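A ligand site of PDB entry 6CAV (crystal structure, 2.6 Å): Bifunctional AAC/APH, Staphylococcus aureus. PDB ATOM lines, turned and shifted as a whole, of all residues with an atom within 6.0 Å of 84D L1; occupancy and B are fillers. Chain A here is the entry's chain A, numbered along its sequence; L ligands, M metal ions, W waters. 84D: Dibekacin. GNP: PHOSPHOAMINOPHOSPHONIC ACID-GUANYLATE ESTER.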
ATOM      1  N   ASN A 199      17.047 -20.761  18.818  1.00  0.00           N
ATOM      2  CA  ASN A 199      18.470 -20.354  18.975  1.00  0.00           C
ATOM      3  C   ASN A 199      19.392 -20.809  17.876  1.00  0.00           C
ATOM      4  O   ASN A 199      20.582 -20.793  18.059  1.00  0.00           O
ATOM      5  CB  ASN A 199      18.984 -20.856  20.349  1.00  0.00           C
ATOM      6  CG  ASN A 199      20.165 -20.079  20.867  1.00  0.00           C
ATOM      7  OD1 ASN A 199      20.419 -18.929  20.484  1.00  0.00           O
ATOM      8  ND2 ASN A 199      20.874 -20.693  21.793  1.00  0.00           N
ATOM      9  N   ASP A 200      18.876 -21.247  16.733  1.00  0.00           N
ATOM     10  CA  ASP A 200      19.702 -21.445  15.542  1.00  0.00           C
ATOM     11  C   ASP A 200      18.805 -21.294  14.321  1.00  0.00           C
ATOM     12  O   ASP A 200      18.756 -22.121  13.412  1.00  0.00           O
ATOM     13  CB  ASP A 200      20.283 -22.788  15.628  1.00  0.00           C
ATOM     14  CG  ASP A 200      21.430 -23.017  14.681  1.00  0.00           C
ATOM     15  OD1 ASP A 200      22.022 -22.082  14.072  1.00  0.00           O
ATOM     16  OD2 ASP A 200      21.753 -24.225  14.551  1.00  0.00           O
ATOM     17  N   PHE A 201      18.071 -20.193  14.323  1.00  0.00           N
ATOM     18  CA  PHE A 201      16.912 -19.991  13.466  1.00  0.00           C
ATOM     19  C   PHE A 201      17.302 -19.374  12.149  1.00  0.00           C
ATOM     20  O   PHE A 201      17.037 -18.223  11.902  1.00  0.00           O
ATOM     21  CB  PHE A 201      15.898 -19.113  14.189  1.00  0.00           C
ATOM     22  CG  PHE A 201      14.501 -19.258  13.680  1.00  0.00           C
ATOM     23  CD1 PHE A 201      13.719 -20.272  14.108  1.00  0.00           C
ATOM     24  CD2 PHE A 201      13.967 -18.359  12.806  1.00  0.00           C
ATOM     25  CE1 PHE A 201      12.454 -20.422  13.636  1.00  0.00           C
ATOM     26  CE2 PHE A 201      12.677 -18.471  12.329  1.00  0.00           C
ATOM     27  CZ  PHE A 201      11.934 -19.502  12.728  1.00  0.00           C
ATOM     28  N   SER A 202      17.903 -20.197  11.306  1.00  0.00           N
ATOM     29  CA  SER A 202      18.462 -19.743  10.028  1.00  0.00           C
ATOM     30  C   SER A 202      17.677 -20.364   8.940  1.00  0.00           C
ATOM     31  O   SER A 202      16.982 -21.354   9.199  1.00  0.00           O
ATOM     32  CB  SER A 202      19.920 -20.193   9.954  1.00  0.00           C
ATOM     33  OG  SER A 202      20.052 -21.515  10.445  1.00  0.00           O
ATOM     34  N   ASN A 204      18.335 -22.345   6.432  1.00  0.00           N
ATOM     35  CA  ASN A 204      18.608 -23.783   6.214  1.00  0.00           C
ATOM     36  C   ASN A 204      17.881 -24.731   7.248  1.00  0.00           C
ATOM     37  O   ASN A 204      18.013 -25.966   7.151  1.00  0.00           O
ATOM     38  CB  ASN A 204      20.093 -24.060   6.193  1.00  0.00           C
ATOM     39  CG  ASN A 204      20.719 -23.937   7.574  1.00  0.00           C
ATOM     40  OD1 ASN A 204      20.647 -22.904   8.174  1.00  0.00           O
ATOM     41  ND2 ASN A 204      21.239 -25.015   8.107  1.00  0.00           N
ATOM     42  N   HIS A 205      17.188 -24.165   8.241  1.00  0.00           N
ATOM     43  CA  HIS A 205      16.349 -24.953   9.129  1.00  0.00           C
ATOM     44  C   HIS A 205      14.846 -24.748   8.906  1.00  0.00           C
ATOM     45  O   HIS A 205      14.042 -25.268   9.635  1.00  0.00           O
ATOM     46  CB  HIS A 205      16.731 -24.660  10.576  1.00  0.00           C
ATOM     47  CG  HIS A 205      18.122 -25.115  10.935  1.00  0.00           C
ATOM     48  ND1 HIS A 205      18.928 -24.424  11.801  1.00  0.00           N
ATOM     49  CD2 HIS A 205      18.833 -26.203  10.545  1.00  0.00           C
ATOM     50  CE1 HIS A 205      20.061 -25.092  11.958  1.00  0.00           C
ATOM     51  NE2 HIS A 205      20.034 -26.181  11.211  1.00  0.00           N
ATOM     52  N   ASP A 219      15.980 -28.771  13.750  1.00  0.00           N
ATOM     53  CA  ASP A 219      17.250 -28.471  14.462  1.00  0.00           C
ATOM     54  C   ASP A 219      17.034 -27.554  15.624  1.00  0.00           C
ATOM     55  O   ASP A 219      17.447 -26.412  15.614  1.00  0.00           O
ATOM     56  CB  ASP A 219      18.347 -27.963  13.537  1.00  0.00           C
ATOM     57  CG  ASP A 219      19.818 -28.103  14.119  1.00  0.00           C
ATOM     58  OD1 ASP A 219      20.026 -28.473  15.315  1.00  0.00           O
ATOM     59  OD2 ASP A 219      20.824 -27.859  13.330  1.00  0.00           O
ATOM     60  N   ASP A 222      20.134 -26.367  19.617  1.00  0.00           N
ATOM     61  CA  ASP A 222      20.727 -25.335  20.418  1.00  0.00           C
ATOM     62  C   ASP A 222      19.685 -24.638  21.302  1.00  0.00           C
ATOM     63  O   ASP A 222      20.016 -23.692  21.999  1.00  0.00           O
ATOM     64  CB  ASP A 222      21.441 -24.361  19.489  1.00  0.00           C
ATOM     65  CG  ASP A 222      22.675 -24.984  18.829  1.00  0.00           C
ATOM     66  OD1 ASP A 222      23.102 -26.114  19.247  1.00  0.00           O
ATOM     67  OD2 ASP A 222      23.229 -24.326  17.924  1.00  0.00           O
ATOM     68  N   TYR A 234      19.792 -14.619  12.914  1.00  0.00           N
ATOM     69  CA  TYR A 234      20.075 -15.057  11.512  1.00  0.00           C
ATOM     70  C   TYR A 234      19.106 -14.423  10.555  1.00  0.00           C
ATOM     71  O   TYR A 234      19.471 -14.122   9.417  1.00  0.00           O
ATOM     72  CB  TYR A 234      20.189 -16.581  11.401  1.00  0.00           C
ATOM     73  CG  TYR A 234      21.311 -17.091  12.271  1.00  0.00           C
ATOM     74  CD1 TYR A 234      22.578 -16.715  12.069  1.00  0.00           C
ATOM     75  CD2 TYR A 234      21.055 -17.907  13.351  1.00  0.00           C
ATOM     76  CE1 TYR A 234      23.634 -17.173  12.897  1.00  0.00           C
ATOM     77  CE2 TYR A 234      22.077 -18.341  14.195  1.00  0.00           C
ATOM     78  CZ  TYR A 234      23.339 -17.976  13.951  1.00  0.00           C
ATOM     79  OH  TYR A 234      24.274 -18.478  14.760  1.00  0.00           O
ATOM     80  N   GLU A 237      20.699 -11.324   9.569  1.00  0.00           N
ATOM     81  CA  GLU A 237      22.081 -11.455   9.072  1.00  0.00           C
ATOM     82  C   GLU A 237      22.159 -11.091   7.619  1.00  0.00           C
ATOM     83  O   GLU A 237      21.343 -11.466   6.813  1.00  0.00           O
ATOM     84  CB  GLU A 237      22.638 -12.847   9.320  1.00  0.00           C
ATOM     85  CG  GLU A 237      23.951 -13.164   8.718  1.00  0.00           C
ATOM     86  CD  GLU A 237      24.401 -14.596   9.019  1.00  0.00           C
ATOM     87  OE1 GLU A 237      24.599 -14.882  10.234  1.00  0.00           O
ATOM     88  OE2 GLU A 237      24.578 -15.404   8.054  1.00  0.00           O
ATOM     89  N   SER A 239      24.339 -11.935   4.683  1.00  0.00           N
ATOM     90  CA  SER A 239      25.319 -12.894   4.195  1.00  0.00           C
ATOM     91  C   SER A 239      24.730 -13.640   3.013  1.00  0.00           C
ATOM     92  O   SER A 239      23.557 -13.497   2.712  1.00  0.00           O
ATOM     93  CB  SER A 239      25.724 -13.892   5.315  1.00  0.00           C
ATOM     94  OG  SER A 239      24.747 -14.873   5.571  1.00  0.00           O
ATOM     95  N   GLU A 241      24.176 -16.804   2.841  1.00  0.00           N
ATOM     96  CA  GLU A 241      23.351 -17.911   3.300  1.00  0.00           C
ATOM     97  C   GLU A 241      21.953 -17.452   3.721  1.00  0.00           C
ATOM     98  O   GLU A 241      21.005 -18.247   3.741  1.00  0.00           O
ATOM     99  CB  GLU A 241      24.012 -18.589   4.491  1.00  0.00           C
ATOM    100  CG  GLU A 241      25.372 -19.187   4.199  1.00  0.00           C
ATOM    101  CD  GLU A 241      26.078 -19.634   5.470  1.00  0.00           C
ATOM    102  OE1 GLU A 241      25.477 -19.664   6.570  1.00  0.00           O
ATOM    103  OE2 GLU A 241      27.272 -19.982   5.359  1.00  0.00           O
ATOM    104  N   GLU A 242      21.838 -16.193   4.130  1.00  0.00           N
ATOM    105  CA  GLU A 242      20.578 -15.694   4.670  1.00  0.00           C
ATOM    106  C   GLU A 242      19.917 -14.694   3.730  1.00  0.00           C
ATOM    107  O   GLU A 242      20.538 -14.188   2.817  1.00  0.00           O
ATOM    108  CB  GLU A 242      20.765 -15.080   6.029  1.00  0.00           C
ATOM    109  CG  GLU A 242      21.427 -15.990   7.048  1.00  0.00           C
ATOM    110  CD  GLU A 242      20.710 -17.279   7.349  1.00  0.00           C
ATOM    111  OE1 GLU A 242      19.458 -17.278   7.386  1.00  0.00           O
ATOM    112  OE2 GLU A 242      21.411 -18.282   7.549  1.00  0.00           O
ATOM    113  N   GLU A 271      27.667 -11.310  15.780  1.00  0.00           N
ATOM    114  CA  GLU A 271      28.439 -11.401  14.542  1.00  0.00           C
ATOM    115  C   GLU A 271      29.900 -11.068  14.857  1.00  0.00           C
ATOM    116  O   GLU A 271      30.802 -11.730  14.354  1.00  0.00           O
ATOM    117  CB  GLU A 271      27.880 -10.486  13.465  1.00  0.00           C
ATOM    118  CG  GLU A 271      28.551 -10.642  12.100  1.00  0.00           C
ATOM    119  CD  GLU A 271      28.382 -12.026  11.503  1.00  0.00           C
ATOM    120  OE1 GLU A 271      29.393 -12.708  11.334  1.00  0.00           O
ATOM    121  OE2 GLU A 271      27.210 -12.461  11.227  1.00  0.00           O
ATOM    122  N   TYR A 274      31.774 -14.063  16.321  1.00  0.00           N
ATOM    123  CA  TYR A 274      31.940 -15.279  15.513  1.00  0.00           C
ATOM    124  C   TYR A 274      33.358 -15.830  15.370  1.00  0.00           C
ATOM    125  O   TYR A 274      33.597 -16.994  15.581  1.00  0.00           O
ATOM    126  CB  TYR A 274      31.279 -15.082  14.149  1.00  0.00           C
ATOM    127  CG  TYR A 274      31.414 -16.257  13.218  1.00  0.00           C
ATOM    128  CD1 TYR A 274      30.729 -17.433  13.452  1.00  0.00           C
ATOM    129  CD2 TYR A 274      32.192 -16.155  12.045  1.00  0.00           C
ATOM    130  CE1 TYR A 274      30.846 -18.490  12.593  1.00  0.00           C
ATOM    131  CE2 TYR A 274      32.309 -17.203  11.166  1.00  0.00           C
ATOM    132  CZ  TYR A 274      31.638 -18.379  11.448  1.00  0.00           C
ATOM    133  OH  TYR A 274      31.717 -19.433  10.593  1.00  0.00           O
ATOM    134  N   GLU A 277      34.414 -17.223  18.697  1.00  0.00           N
ATOM    135  CA  GLU A 277      33.682 -18.465  18.914  1.00  0.00           C
ATOM    136  C   GLU A 277      34.361 -19.619  18.145  1.00  0.00           C
ATOM    137  O   GLU A 277      34.426 -20.716  18.636  1.00  0.00           O
ATOM    138  CB  GLU A 277      32.214 -18.320  18.451  1.00  0.00           C
ATOM    139  CG  GLU A 277      31.340 -19.480  18.918  1.00  0.00           C
ATOM    140  CD  GLU A 277      29.880 -19.363  18.512  1.00  0.00           C
ATOM    141  OE1 GLU A 277      29.619 -18.945  17.365  1.00  0.00           O
ATOM    142  OE2 GLU A 277      29.023 -19.750  19.350  1.00  0.00           O
ATOM    143  N   THR A 278      34.821 -19.326  16.938  1.00  0.00           N
ATOM    144  CA  THR A 278      35.456 -20.284  16.091  1.00  0.00           C
ATOM    145  C   THR A 278      36.790 -20.712  16.714  1.00  0.00           C
ATOM    146  O   THR A 278      37.089 -21.934  16.785  1.00  0.00           O
ATOM    147  CB  THR A 278      35.646 -19.741  14.662  1.00  0.00           C
ATOM    148  OG1 THR A 278      34.362 -19.350  14.143  1.00  0.00           O
ATOM    149  CG2 THR A 278      36.250 -20.795  13.744  1.00  0.00           C
HETATM  150  C1  84D L   1      27.944 -15.808   9.125  1.00  0.00           C
HETATM  151  C2  84D L   1      28.221 -16.367  10.511  1.00  0.00           C
HETATM  152  C3  84D L   1      27.950 -17.856  10.439  1.00  0.00           C
HETATM  153  O3  84D L   1      25.161 -21.769  12.688  1.00  0.00           O
HETATM  154  C4  84D L   1      28.406 -18.029   8.050  1.00  0.00           C
HETATM  155  O4  84D L   1      27.016 -22.175  13.665  1.00  0.00           O
HETATM  156  C5  84D L   1      29.433 -18.802   7.254  1.00  0.00           C
HETATM  157  O5  84D L   1      28.650 -20.694  14.964  1.00  0.00           O
HETATM  158  C6  84D L   1      25.867 -19.226  10.134  1.00  0.00           C
HETATM  159  O6  84D L   1      25.908 -23.135  16.986  1.00  0.00           O
HETATM  160  C7  84D L   1      24.439 -18.908   9.677  1.00  0.00           C
HETATM  161  O7  84D L   1      24.555 -24.649  12.381  1.00  0.00           O
HETATM  162  C8  84D L   1      23.545 -20.128   9.828  1.00  0.00           C
HETATM  163  C9  84D L   1      23.586 -20.707  11.231  1.00  0.00           C
HETATM  164  C10 84D L   1      25.021 -21.098  11.446  1.00  0.00           C
HETATM  165  C11 84D L   1      25.874 -19.853  11.520  1.00  0.00           C
HETATM  166  C12 84D L   1      26.107 -22.774  12.756  1.00  0.00           C
HETATM  167  C13 84D L   1      25.501 -24.062  13.307  1.00  0.00           C
HETATM  168  C14 84D L   1      24.961 -23.712  14.713  1.00  0.00           C
HETATM  169  N1  84D L   1      24.148 -24.734  15.377  1.00  0.00           N
HETATM  170  C15 84D L   1      26.160 -23.322  15.597  1.00  0.00           C
HETATM  171  C16 84D L   1      26.591 -21.988  15.031  1.00  0.00           C
HETATM  172  C17 84D L   1      27.765 -21.428  15.804  1.00  0.00           C
HETATM  173  N2  84D L   1      22.700 -21.859  11.434  1.00  0.00           N
HETATM  174  N3  84D L   1      24.388 -18.401   8.296  1.00  0.00           N
HETATM  175  O2  84D L   1      27.146 -20.226  12.035  1.00  0.00           O
HETATM  176  O1  84D L   1      26.565 -17.969  10.148  1.00  0.00           O
HETATM  177  N4  84D L   1      27.328 -15.704  11.475  1.00  0.00           N
HETATM  178  O   84D L   1      28.721 -18.411   9.399  1.00  0.00           O
HETATM  179  C   84D L   1      28.517 -16.529   7.901  1.00  0.00           C
HETATM  180  N   84D L   1      29.161 -20.222   7.152  1.00  0.00           N
HETATM  181  PG  GNP L   2      23.579 -30.639  15.095  1.00  0.00           P
HETATM  182  O1G GNP L   2      23.671 -31.703  16.241  1.00  0.00           O
HETATM  183  O2G GNP L   2      24.798 -29.826  15.054  1.00  0.00           O
HETATM  184  O3G GNP L   2      22.177 -29.795  15.111  1.00  0.00           O
HETATM  185  N3B GNP L   2      23.481 -31.376  13.648  1.00  0.00           N
HETATM  186  PB  GNP L   2      22.968 -30.733  12.245  1.00  0.00           P
HETATM  187  O1B GNP L   2      23.877 -31.203  11.105  1.00  0.00           O
HETATM  188  O2B GNP L   2      22.783 -29.300  12.279  1.00  0.00           O
HETATM  189  O3A GNP L   2      21.488 -31.338  12.095  1.00  0.00           O
HETATM  190  PA  GNP L   2      20.099 -30.892  11.441  1.00  0.00           P
HETATM  191  O1A GNP L   2      19.088 -31.044  12.615  1.00  0.00           O
HETATM  192  O2A GNP L   2      20.221 -29.492  11.000  1.00  0.00           O
HETATM  193  O5' GNP L   2      19.960 -31.837  10.177  1.00  0.00           O
HETATM  194  C5' GNP L   2      21.043 -31.857   9.249  1.00  0.00           C
HETATM  195  C4' GNP L   2      20.435 -31.668   7.885  1.00  0.00           C
HETATM  196  O4' GNP L   2      19.620 -32.830   7.639  1.00  0.00           O
HETATM  197  C3' GNP L   2      19.460 -30.522   7.713  1.00  0.00           C
HETATM  198  O3' GNP L   2      20.086 -29.311   7.335  1.00  0.00           O
HETATM  199  C2' GNP L   2      18.623 -31.012   6.549  1.00  0.00           C
HETATM  200  O2' GNP L   2      19.351 -31.055   5.347  1.00  0.00           O
HETATM  201  C1' GNP L   2      18.454 -32.481   6.919  1.00  0.00           C
HETATM  202  N9  GNP L   2      17.227 -32.812   7.762  1.00  0.00           N
HETATM  203  C8  GNP L   2      17.091 -33.004   9.116  1.00  0.00           C
HETATM  204  N7  GNP L   2      15.898 -33.286   9.458  1.00  0.00           N
HETATM  205  C5  GNP L   2      15.196 -33.245   8.265  1.00  0.00           C
HETATM  206  C6  GNP L   2      13.867 -33.252   8.026  1.00  0.00           C
HETATM  207  O6  GNP L   2      13.000 -33.401   8.878  1.00  0.00           O
HETATM  208  N1  GNP L   2      13.518 -32.958   6.706  1.00  0.00           N
HETATM  209  C2  GNP L   2      14.388 -32.756   5.711  1.00  0.00           C
HETATM  210  N2  GNP L   2      13.875 -32.350   4.535  1.00  0.00           N
HETATM  211  N3  GNP L   2      15.684 -32.816   5.896  1.00  0.00           N
HETATM  212  C4  GNP L   2      16.019 -33.016   7.195  1.00  0.00           C
HETATM  213 MG    MG M   1      22.276 -27.863  15.153  1.00  0.00          MG
HETATM  214 MG    MG M   2      21.659 -27.773  11.637  1.00  0.00          MG
HETATM  215  O   HOH W   1      26.808 -16.884  14.034  1.00  0.00           O
HETATM  216  O   HOH W   2      21.161 -26.401  16.083  1.00  0.00           O
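N of Glu 241 sits close to OG of Ser 239.
O of Asp 200 is in hydrogen-bond range of OG of Ser 202, 3.3 Å away.
O of Tyr 274 sits at hydrogen-bond distance from OG1 of Thr 278.
The side-chain hydroxyl (OG) of Ser 202 is in hydrogen-bond range of a ring nitrogen (ND1) of His 205, 3.4 Å away.
The side-chain amide nitrogen (ND2) of Asn 199 lies within hydrogen-bond range of the backbone carbonyl oxygen (O) of Asp 222, at 3.1 Å.
OD1 of Asn 204 lies within hydrogen-bond range of OG of Ser 202 (2.7 Å).
The backbone carbonyl oxygen (O) of Asp 200 is in hydrogen-bond range of a ring nitrogen (ND1) of His 205.
OG of Ser 239 sits at hydrogen-bond distance from OE2 of Glu 237.
Water W1 lies within hydrogen-bond range of a nitrogen (N4) of 84D L1 (2.9 Å) and the side-chain hydroxyl of Tyr 234 (3.1 Å).
Water W2 lies within hydrogen-bond range of OD2 of Asp 200 (2.7 Å), OD2 of Asp 222 (3.5 Å) and N1 of 84D L1 (3.5 Å).
OH of Tyr 274 lies within hydrogen-bond range of O of 84D L1 (3.4 Å).
The side-chain hydroxyl of Ser 202 is in hydrogen-bond range of a nitrogen (N2) of 84D L1 (2.8 Å).
The side-chain carboxylate of Glu 277 is in hydrogen-bond range of an oxygen (O5) of 84D L1.
OD2 of Asp 222 lies within salt-bridge range of N1 of 84D L1 (2.7 Å).
The side-chain carboxylate of Glu 241 lies within salt-bridge range of a nitrogen (N3) of 84D L1, at 2.4 Å.
A nitrogen (N4) of 84D L1 is in salt-bridge range of the side-chain carboxylate of Glu 271 (3.3 Å).
N3 of 84D L1 is in salt-bridge range of OE2 of Glu 237 (3.0 Å).
OD2 of Asp 200 is in salt-bridge range of N1 of 84D L1 (2.6 Å).
The side-chain carboxylate (OE2) of Glu 242 lies within salt-bridge range of a nitrogen (N3) of 84D L1 (3.1 Å).
Residues that only touch 84D L1: Asn 204 (3.99 Å) and Tyr 234 (3.7 Å).
Hydrophobic or aromatic side chains within 4 Å of 84D L1: Tyr 234 and Tyr 274.
Within 4 Å of 84D L1: Asp 200, Ser 202, Asn 204, Asp 222, Tyr 234, Glu 237, Glu 241, Glu 242, Glu 271, Tyr 274 and Glu 277.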
